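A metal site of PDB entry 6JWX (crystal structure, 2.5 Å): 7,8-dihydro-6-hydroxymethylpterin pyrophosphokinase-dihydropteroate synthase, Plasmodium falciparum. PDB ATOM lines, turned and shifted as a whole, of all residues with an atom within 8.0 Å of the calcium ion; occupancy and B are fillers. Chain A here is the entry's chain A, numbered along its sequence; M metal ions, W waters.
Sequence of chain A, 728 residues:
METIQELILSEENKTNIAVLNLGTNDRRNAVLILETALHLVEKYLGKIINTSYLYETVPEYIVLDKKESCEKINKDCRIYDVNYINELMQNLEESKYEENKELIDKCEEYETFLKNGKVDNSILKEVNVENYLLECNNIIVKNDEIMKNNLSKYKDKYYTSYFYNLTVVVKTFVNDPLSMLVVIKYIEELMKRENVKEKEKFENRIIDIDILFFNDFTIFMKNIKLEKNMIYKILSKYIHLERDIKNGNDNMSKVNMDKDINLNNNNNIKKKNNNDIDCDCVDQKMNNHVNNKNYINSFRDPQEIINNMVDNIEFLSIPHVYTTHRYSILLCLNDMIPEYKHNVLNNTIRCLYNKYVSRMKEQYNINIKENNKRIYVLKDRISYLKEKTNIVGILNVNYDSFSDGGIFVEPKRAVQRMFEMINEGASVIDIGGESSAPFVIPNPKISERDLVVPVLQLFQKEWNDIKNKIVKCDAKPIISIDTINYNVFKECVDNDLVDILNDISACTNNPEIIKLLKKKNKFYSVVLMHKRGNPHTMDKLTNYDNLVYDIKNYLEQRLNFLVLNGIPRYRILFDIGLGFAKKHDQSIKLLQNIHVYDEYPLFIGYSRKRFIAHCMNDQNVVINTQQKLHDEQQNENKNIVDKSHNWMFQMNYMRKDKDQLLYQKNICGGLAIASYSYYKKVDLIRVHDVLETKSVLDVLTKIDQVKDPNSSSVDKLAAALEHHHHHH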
ATOM      1  N   LEU A  38      20.770 -15.002 -27.326  1.00  0.00           N
ATOM      2  CA  LEU A  38      21.311 -14.096 -28.358  1.00  0.00           C
ATOM      3  C   LEU A  38      20.462 -12.854 -28.506  1.00  0.00           C
ATOM      4  O   LEU A  38      21.003 -11.760 -28.567  1.00  0.00           O
ATOM      5  CB  LEU A  38      21.490 -14.770 -29.720  1.00  0.00           C
ATOM      6  CG  LEU A  38      22.610 -15.799 -29.901  1.00  0.00           C
ATOM      7  CD1 LEU A  38      22.664 -16.201 -31.364  1.00  0.00           C
ATOM      8  CD2 LEU A  38      23.951 -15.241 -29.432  1.00  0.00           C
ATOM      9  N   HIS A  39      19.138 -13.013 -28.517  1.00  0.00           N
ATOM     10  CA  HIS A  39      18.269 -11.837 -28.636  1.00  0.00           C
ATOM     11  C   HIS A  39      18.341 -10.920 -27.445  1.00  0.00           C
ATOM     12  O   HIS A  39      18.273  -9.713 -27.617  1.00  0.00           O
ATOM     13  CB  HIS A  39      16.797 -12.166 -28.923  1.00  0.00           C
ATOM     14  CG  HIS A  39      15.939 -10.934 -29.003  1.00  0.00           C
ATOM     15  ND1 HIS A  39      16.214  -9.881 -29.861  1.00  0.00           N
ATOM     16  CD2 HIS A  39      14.843 -10.552 -28.295  1.00  0.00           C
ATOM     17  CE1 HIS A  39      15.313  -8.927 -29.686  1.00  0.00           C
ATOM     18  NE2 HIS A  39      14.471  -9.311 -28.748  1.00  0.00           N
ATOM     19  N   LEU A  40      18.439 -11.481 -26.245  1.00  0.00           N
ATOM     20  CA  LEU A  40      18.505 -10.683 -25.025  1.00  0.00           C
ATOM     21  C   LEU A  40      19.833  -9.937 -24.972  1.00  0.00           C
ATOM     22  O   LEU A  40      19.861  -8.788 -24.526  1.00  0.00           O
ATOM     23  CB  LEU A  40      18.213 -11.511 -23.775  1.00  0.00           C
ATOM     24  CG  LEU A  40      16.800 -12.138 -23.768  1.00  0.00           C
ATOM     25  CD1 LEU A  40      16.541 -13.018 -22.556  1.00  0.00           C
ATOM     26  CD2 LEU A  40      15.677 -11.118 -23.895  1.00  0.00           C
ATOM     27  N   VAL A  41      20.888 -10.558 -25.495  1.00  0.00           N
ATOM     28  CA  VAL A  41      22.181  -9.909 -25.686  1.00  0.00           C
ATOM     29  C   VAL A  41      22.123  -8.712 -26.647  1.00  0.00           C
ATOM     30  O   VAL A  41      22.635  -7.659 -26.285  1.00  0.00           O
ATOM     31  CB  VAL A  41      23.301 -10.912 -26.041  1.00  0.00           C
ATOM     32  CG1 VAL A  41      24.594 -10.199 -26.451  1.00  0.00           C
ATOM     33  CG2 VAL A  41      23.574 -11.848 -24.873  1.00  0.00           C
ATOM     34  N   GLU A  42      21.478  -8.856 -27.826  1.00  0.00           N
ATOM     35  CA  GLU A  42      21.281  -7.706 -28.759  1.00  0.00           C
ATOM     36  C   GLU A  42      20.471  -6.611 -28.130  1.00  0.00           C
ATOM     37  O   GLU A  42      20.713  -5.420 -28.380  1.00  0.00           O
ATOM     38  CB  GLU A  42      20.542  -8.080 -30.060  1.00  0.00           C
ATOM     39  CG  GLU A  42      21.415  -8.412 -31.245  1.00  0.00           C
ATOM     40  CD  GLU A  42      22.109  -7.220 -31.910  1.00  0.00           C
ATOM     41  OE1 GLU A  42      21.788  -6.018 -31.645  1.00  0.00           O
ATOM     42  OE2 GLU A  42      23.010  -7.531 -32.728  1.00  0.00           O
ATOM     43  N   LYS A  43      19.472  -7.021 -27.348  1.00  0.00           N
ATOM     44  CA  LYS A  43      18.552  -6.085 -26.715  1.00  0.00           C
ATOM     45  C   LYS A  43      19.224  -5.345 -25.567  1.00  0.00           C
ATOM     46  O   LYS A  43      19.220  -4.129 -25.574  1.00  0.00           O
ATOM     47  CB  LYS A  43      17.310  -6.831 -26.230  1.00  0.00           C
ATOM     48  CG  LYS A  43      16.141  -5.961 -25.843  1.00  0.00           C
ATOM     49  CD  LYS A  43      15.031  -6.858 -25.311  1.00  0.00           C
ATOM     50  CE  LYS A  43      13.824  -6.027 -24.874  1.00  0.00           C
ATOM     51  NZ  LYS A  43      13.035  -5.455 -25.991  1.00  0.00           N
ATOM     52  N   TYR A  44      19.803  -6.078 -24.611  1.00  0.00           N
ATOM     53  CA  TYR A  44      20.227  -5.474 -23.355  1.00  0.00           C
ATOM     54  C   TYR A  44      21.693  -5.104 -23.260  1.00  0.00           C
ATOM     55  O   TYR A  44      22.063  -4.267 -22.457  1.00  0.00           O
ATOM     56  CB  TYR A  44      19.826  -6.328 -22.149  1.00  0.00           C
ATOM     57  CG  TYR A  44      18.328  -6.447 -21.928  1.00  0.00           C
ATOM     58  CD1 TYR A  44      17.490  -5.323 -21.989  1.00  0.00           C
ATOM     59  CD2 TYR A  44      17.748  -7.674 -21.650  1.00  0.00           C
ATOM     60  CE1 TYR A  44      16.126  -5.435 -21.787  1.00  0.00           C
ATOM     61  CE2 TYR A  44      16.382  -7.800 -21.457  1.00  0.00           C
ATOM     62  CZ  TYR A  44      15.580  -6.683 -21.520  1.00  0.00           C
ATOM     63  OH  TYR A  44      14.214  -6.808 -21.327  1.00  0.00           O
ATOM     64  N   LEU A  45      22.553  -5.710 -24.091  1.00  0.00           N
ATOM     65  CA  LEU A  45      23.988  -5.521 -23.928  1.00  0.00           C
ATOM     66  C   LEU A  45      24.698  -4.672 -24.989  1.00  0.00           C
ATOM     67  O   LEU A  45      25.687  -4.036 -24.686  1.00  0.00           O
ATOM     68  CB  LEU A  45      24.699  -6.865 -23.725  1.00  0.00           C
ATOM     69  CG  LEU A  45      24.221  -7.636 -22.503  1.00  0.00           C
ATOM     70  CD1 LEU A  45      24.835  -9.025 -22.403  1.00  0.00           C
ATOM     71  CD2 LEU A  45      24.479  -6.833 -21.233  1.00  0.00           C
ATOM     72  N   GLY A  46      24.186  -4.660 -26.217  1.00  0.00           N
ATOM     73  CA  GLY A  46      24.871  -3.953 -27.312  1.00  0.00           C
ATOM     74  C   GLY A  46      24.628  -4.643 -28.629  1.00  0.00           C
ATOM     75  O   GLY A  46      23.551  -5.175 -28.881  1.00  0.00           O
ATOM     76  N   LYS A  47      25.648  -4.674 -29.467  1.00  0.00           N
ATOM     77  CA  LYS A  47      25.523  -5.279 -30.787  1.00  0.00           C
ATOM     78  C   LYS A  47      26.323  -6.577 -30.854  1.00  0.00           C
ATOM     79  O   LYS A  47      27.462  -6.615 -30.396  1.00  0.00           O
ATOM     80  CB  LYS A  47      25.997  -4.281 -31.872  1.00  0.00           C
ATOM     81  CG  LYS A  47      25.734  -4.771 -33.280  1.00  0.00           C
ATOM     82  CD  LYS A  47      26.195  -3.785 -34.332  1.00  0.00           C
ATOM     83  CE  LYS A  47      25.776  -4.242 -35.721  1.00  0.00           C
ATOM     84  NZ  LYS A  47      24.360  -4.711 -35.747  1.00  0.00           N
ATOM     85  N   ILE A  48      25.728  -7.622 -31.420  1.00  0.00           N
ATOM     86  CA  ILE A  48      26.416  -8.885 -31.693  1.00  0.00           C
ATOM     87  C   ILE A  48      27.163  -8.728 -33.027  1.00  0.00           C
ATOM     88  O   ILE A  48      26.549  -8.467 -34.051  1.00  0.00           O
ATOM     89  CB  ILE A  48      25.429 -10.082 -31.744  1.00  0.00           C
ATOM     90  CG1 ILE A  48      24.845 -10.352 -30.354  1.00  0.00           C
ATOM     91  CG2 ILE A  48      26.094 -11.354 -32.288  1.00  0.00           C
ATOM     92  CD1 ILE A  48      23.876 -11.524 -30.271  1.00  0.00           C
ATOM     93  N   SER A  95      14.953  -1.736 -23.294  1.00  0.00           N
ATOM     94  CA  SER A  95      16.311  -1.272 -23.015  1.00  0.00           C
ATOM     95  C   SER A  95      16.299   0.244 -23.074  1.00  0.00           C
ATOM     96  O   SER A  95      15.493   0.830 -23.800  1.00  0.00           O
ATOM     97  CB  SER A  95      17.298  -1.814 -24.039  1.00  0.00           C
ATOM     98  OG  SER A  95      18.520  -1.083 -23.996  1.00  0.00           O
ATOM     99  N   TYR A  97      18.810   1.723 -24.250  1.00  0.00           N
ATOM    100  CA  TYR A  97      19.710   1.978 -25.369  1.00  0.00           C
ATOM    101  C   TYR A  97      19.065   1.514 -26.649  1.00  0.00           C
ATOM    102  O   TYR A  97      18.395   0.463 -26.675  1.00  0.00           O
ATOM    103  CB  TYR A  97      21.065   1.297 -25.153  1.00  0.00           C
ATOM    104  CG  TYR A  97      21.896   1.950 -24.091  1.00  0.00           C
ATOM    105  CD1 TYR A  97      21.576   1.791 -22.734  1.00  0.00           C
ATOM    106  CD2 TYR A  97      22.999   2.755 -24.423  1.00  0.00           C
ATOM    107  CE1 TYR A  97      22.316   2.419 -21.753  1.00  0.00           C
ATOM    108  CE2 TYR A  97      23.758   3.378 -23.430  1.00  0.00           C
ATOM    109  CZ  TYR A  97      23.395   3.198 -22.092  1.00  0.00           C
ATOM    110  OH  TYR A  97      24.090   3.783 -21.066  1.00  0.00           O
ATOM    111  N   GLU A  98      19.266   2.280 -27.708  1.00  0.00           N
ATOM    112  CA  GLU A  98      18.524   2.045 -28.942  1.00  0.00           C
ATOM    113  C   GLU A  98      19.111   0.934 -29.804  1.00  0.00           C
ATOM    114  O   GLU A  98      20.323   0.761 -29.896  1.00  0.00           O
ATOM    115  CB  GLU A  98      18.295   3.355 -29.737  1.00  0.00           C
ATOM    116  CG  GLU A  98      19.424   3.829 -30.652  1.00  0.00           C
ATOM    117  CD  GLU A  98      20.522   4.608 -29.957  1.00  0.00           C
ATOM    118  OE1 GLU A  98      20.404   4.890 -28.736  1.00  0.00           O
ATOM    119  OE2 GLU A  98      21.518   4.951 -30.651  1.00  0.00           O
ATOM    120  N   GLU A  99      18.219   0.143 -30.375  1.00  0.00           N
ATOM    121  CA  GLU A  99      18.601  -0.790 -31.405  1.00  0.00           C
ATOM    122  C   GLU A  99      18.922  -0.018 -32.705  1.00  0.00           C
ATOM    123  O   GLU A  99      18.337   1.048 -32.985  1.00  0.00           O
ATOM    124  CB  GLU A  99      17.474  -1.794 -31.626  1.00  0.00           C
ATOM    125  CG  GLU A  99      17.876  -3.100 -32.290  1.00  0.00           C
ATOM    126  CD  GLU A  99      19.141  -3.709 -31.707  1.00  0.00           C
ATOM    127  OE1 GLU A  99      20.241  -3.432 -32.252  1.00  0.00           O
ATOM    128  OE2 GLU A  99      19.056  -4.461 -30.703  1.00  0.00           O
ATOM    129  N   ASN A 100      19.886  -0.546 -33.461  1.00  0.00           N
ATOM    130  CA  ASN A 100      20.223  -0.046 -34.784  1.00  0.00           C
ATOM    131  C   ASN A 100      20.462  -1.270 -35.626  1.00  0.00           C
ATOM    132  O   ASN A 100      21.312  -2.081 -35.299  1.00  0.00           O
ATOM    133  CB  ASN A 100      21.473   0.845 -34.746  1.00  0.00           C
ATOM    134  CG  ASN A 100      21.243   2.180 -34.049  1.00  0.00           C
ATOM    135  OD1 ASN A 100      20.181   2.795 -34.171  1.00  0.00           O
ATOM    136  ND2 ASN A 100      22.251   2.660 -33.335  1.00  0.00           N
ATOM    137  N   LYS A 101      19.689  -1.451 -36.691  1.00  0.00           N
ATOM    138  CA  LYS A 101      19.824  -2.642 -37.530  1.00  0.00           C
ATOM    139  C   LYS A 101      20.622  -2.330 -38.795  1.00  0.00           C
ATOM    140  O   LYS A 101      20.894  -3.207 -39.594  1.00  0.00           O
ATOM    141  CB  LYS A 101      18.467  -3.224 -37.907  1.00  0.00           C
ATOM    142  CG  LYS A 101      17.628  -3.719 -36.734  1.00  0.00           C
ATOM    143  CD  LYS A 101      16.442  -4.549 -37.205  1.00  0.00           C
ATOM    144  CE  LYS A 101      16.930  -5.824 -37.899  1.00  0.00           C
ATOM    145  NZ  LYS A 101      15.852  -6.748 -38.304  1.00  0.00           N
ATOM    146  N   VAL A 170      30.343  -9.096 -28.426  1.00  0.00           N
ATOM    147  CA  VAL A 170      29.427  -7.996 -28.252  1.00  0.00           C
ATOM    148  C   VAL A 170      30.184  -6.666 -28.182  1.00  0.00           C
ATOM    149  O   VAL A 170      31.122  -6.512 -27.406  1.00  0.00           O
ATOM    150  CB  VAL A 170      28.529  -8.164 -27.002  1.00  0.00           C
ATOM    151  CG1 VAL A 170      27.408  -7.132 -27.001  1.00  0.00           C
ATOM    152  CG2 VAL A 170      27.931  -9.564 -26.984  1.00  0.00           C
ATOM    153  N   LYS A 171      29.758  -5.741 -29.020  1.00  0.00           N
ATOM    154  CA  LYS A 171      30.116  -4.348 -28.925  1.00  0.00           C
ATOM    155  C   LYS A 171      29.113  -3.785 -27.927  1.00  0.00           C
ATOM    156  O   LYS A 171      27.929  -3.594 -28.264  1.00  0.00           O
ATOM    157  CB  LYS A 171      29.966  -3.701 -30.298  1.00  0.00           C
ATOM    158  CG  LYS A 171      30.637  -2.364 -30.494  1.00  0.00           C
ATOM    159  CD  LYS A 171      29.947  -1.624 -31.647  1.00  0.00           C
ATOM    160  CE  LYS A 171      30.900  -0.733 -32.435  1.00  0.00           C
ATOM    161  NZ  LYS A 171      30.683  -0.968 -33.888  1.00  0.00           N
ATOM    162  N   PHE A 173      27.527  -1.294 -24.712  1.00  0.00           N
ATOM    163  CA  PHE A 173      27.420   0.043 -24.075  1.00  0.00           C
ATOM    164  C   PHE A 173      27.548  -0.045 -22.549  1.00  0.00           C
ATOM    165  O   PHE A 173      27.497   0.960 -21.847  1.00  0.00           O
ATOM    166  CB  PHE A 173      26.102   0.734 -24.462  1.00  0.00           C
ATOM    167  CG  PHE A 173      24.904  -0.181 -24.428  1.00  0.00           C
ATOM    168  CD1 PHE A 173      24.372  -0.611 -23.214  1.00  0.00           C
ATOM    169  CD2 PHE A 173      24.311  -0.603 -25.630  1.00  0.00           C
ATOM    170  CE1 PHE A 173      23.286  -1.488 -23.197  1.00  0.00           C
ATOM    171  CE2 PHE A 173      23.229  -1.466 -25.603  1.00  0.00           C
ATOM    172  CZ  PHE A 173      22.726  -1.914 -24.391  1.00  0.00           C
ATOM    173  N   LYS A 518      16.988 -11.348 -39.339  1.00  0.00           N
ATOM    174  CA  LYS A 518      16.788 -11.170 -37.899  1.00  0.00           C
ATOM    175  C   LYS A 518      15.382 -10.627 -37.690  1.00  0.00           C
ATOM    176  O   LYS A 518      15.043  -9.565 -38.181  1.00  0.00           O
ATOM    177  CB  LYS A 518      17.819 -10.212 -37.282  1.00  0.00           C
ATOM    178  CG  LYS A 518      19.274 -10.477 -37.623  1.00  0.00           C
ATOM    179  CD  LYS A 518      20.053  -9.180 -37.876  1.00  0.00           C
ATOM    180  CE  LYS A 518      20.787  -8.704 -36.619  1.00  0.00           C
ATOM    181  NZ  LYS A 518      20.856  -7.205 -36.531  1.00  0.00           N
HETATM  182 CA    CA M   1      21.424  -4.063 -30.104  1.00  0.00          CA
HETATM  183  O   HOH W   1      23.207  -2.750 -30.801  1.00  0.00           O
HETATM  184  O   HOH W   2      20.187  -2.225 -28.301  1.00  0.00           O
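The side-chain carboxylate (OE2) of Glu 42 lies within hydrogen-bond range of the backbone NH (N) of Ile 48. The backbone NH (N) of Gly 46 is in hydrogen-bond range of the backbone carbonyl oxygen (O) of Val 41, at 3.4 Å.
Water W2 bridges the backbone carbonyl oxygen (O) of Glu 98 (3.4 Å) and the backbone carbonyl oxygen (O) of Lys 43 (3.5 Å).
Of the 21 residues printed, 3 come within 4 Å of the calcium ion.
The calcium ion is bound by O of Glu 42, water W1, OE2 of Glu 99, OE1 of Glu 42, OE1 of Glu 99, O of Gly 46 and water W2.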
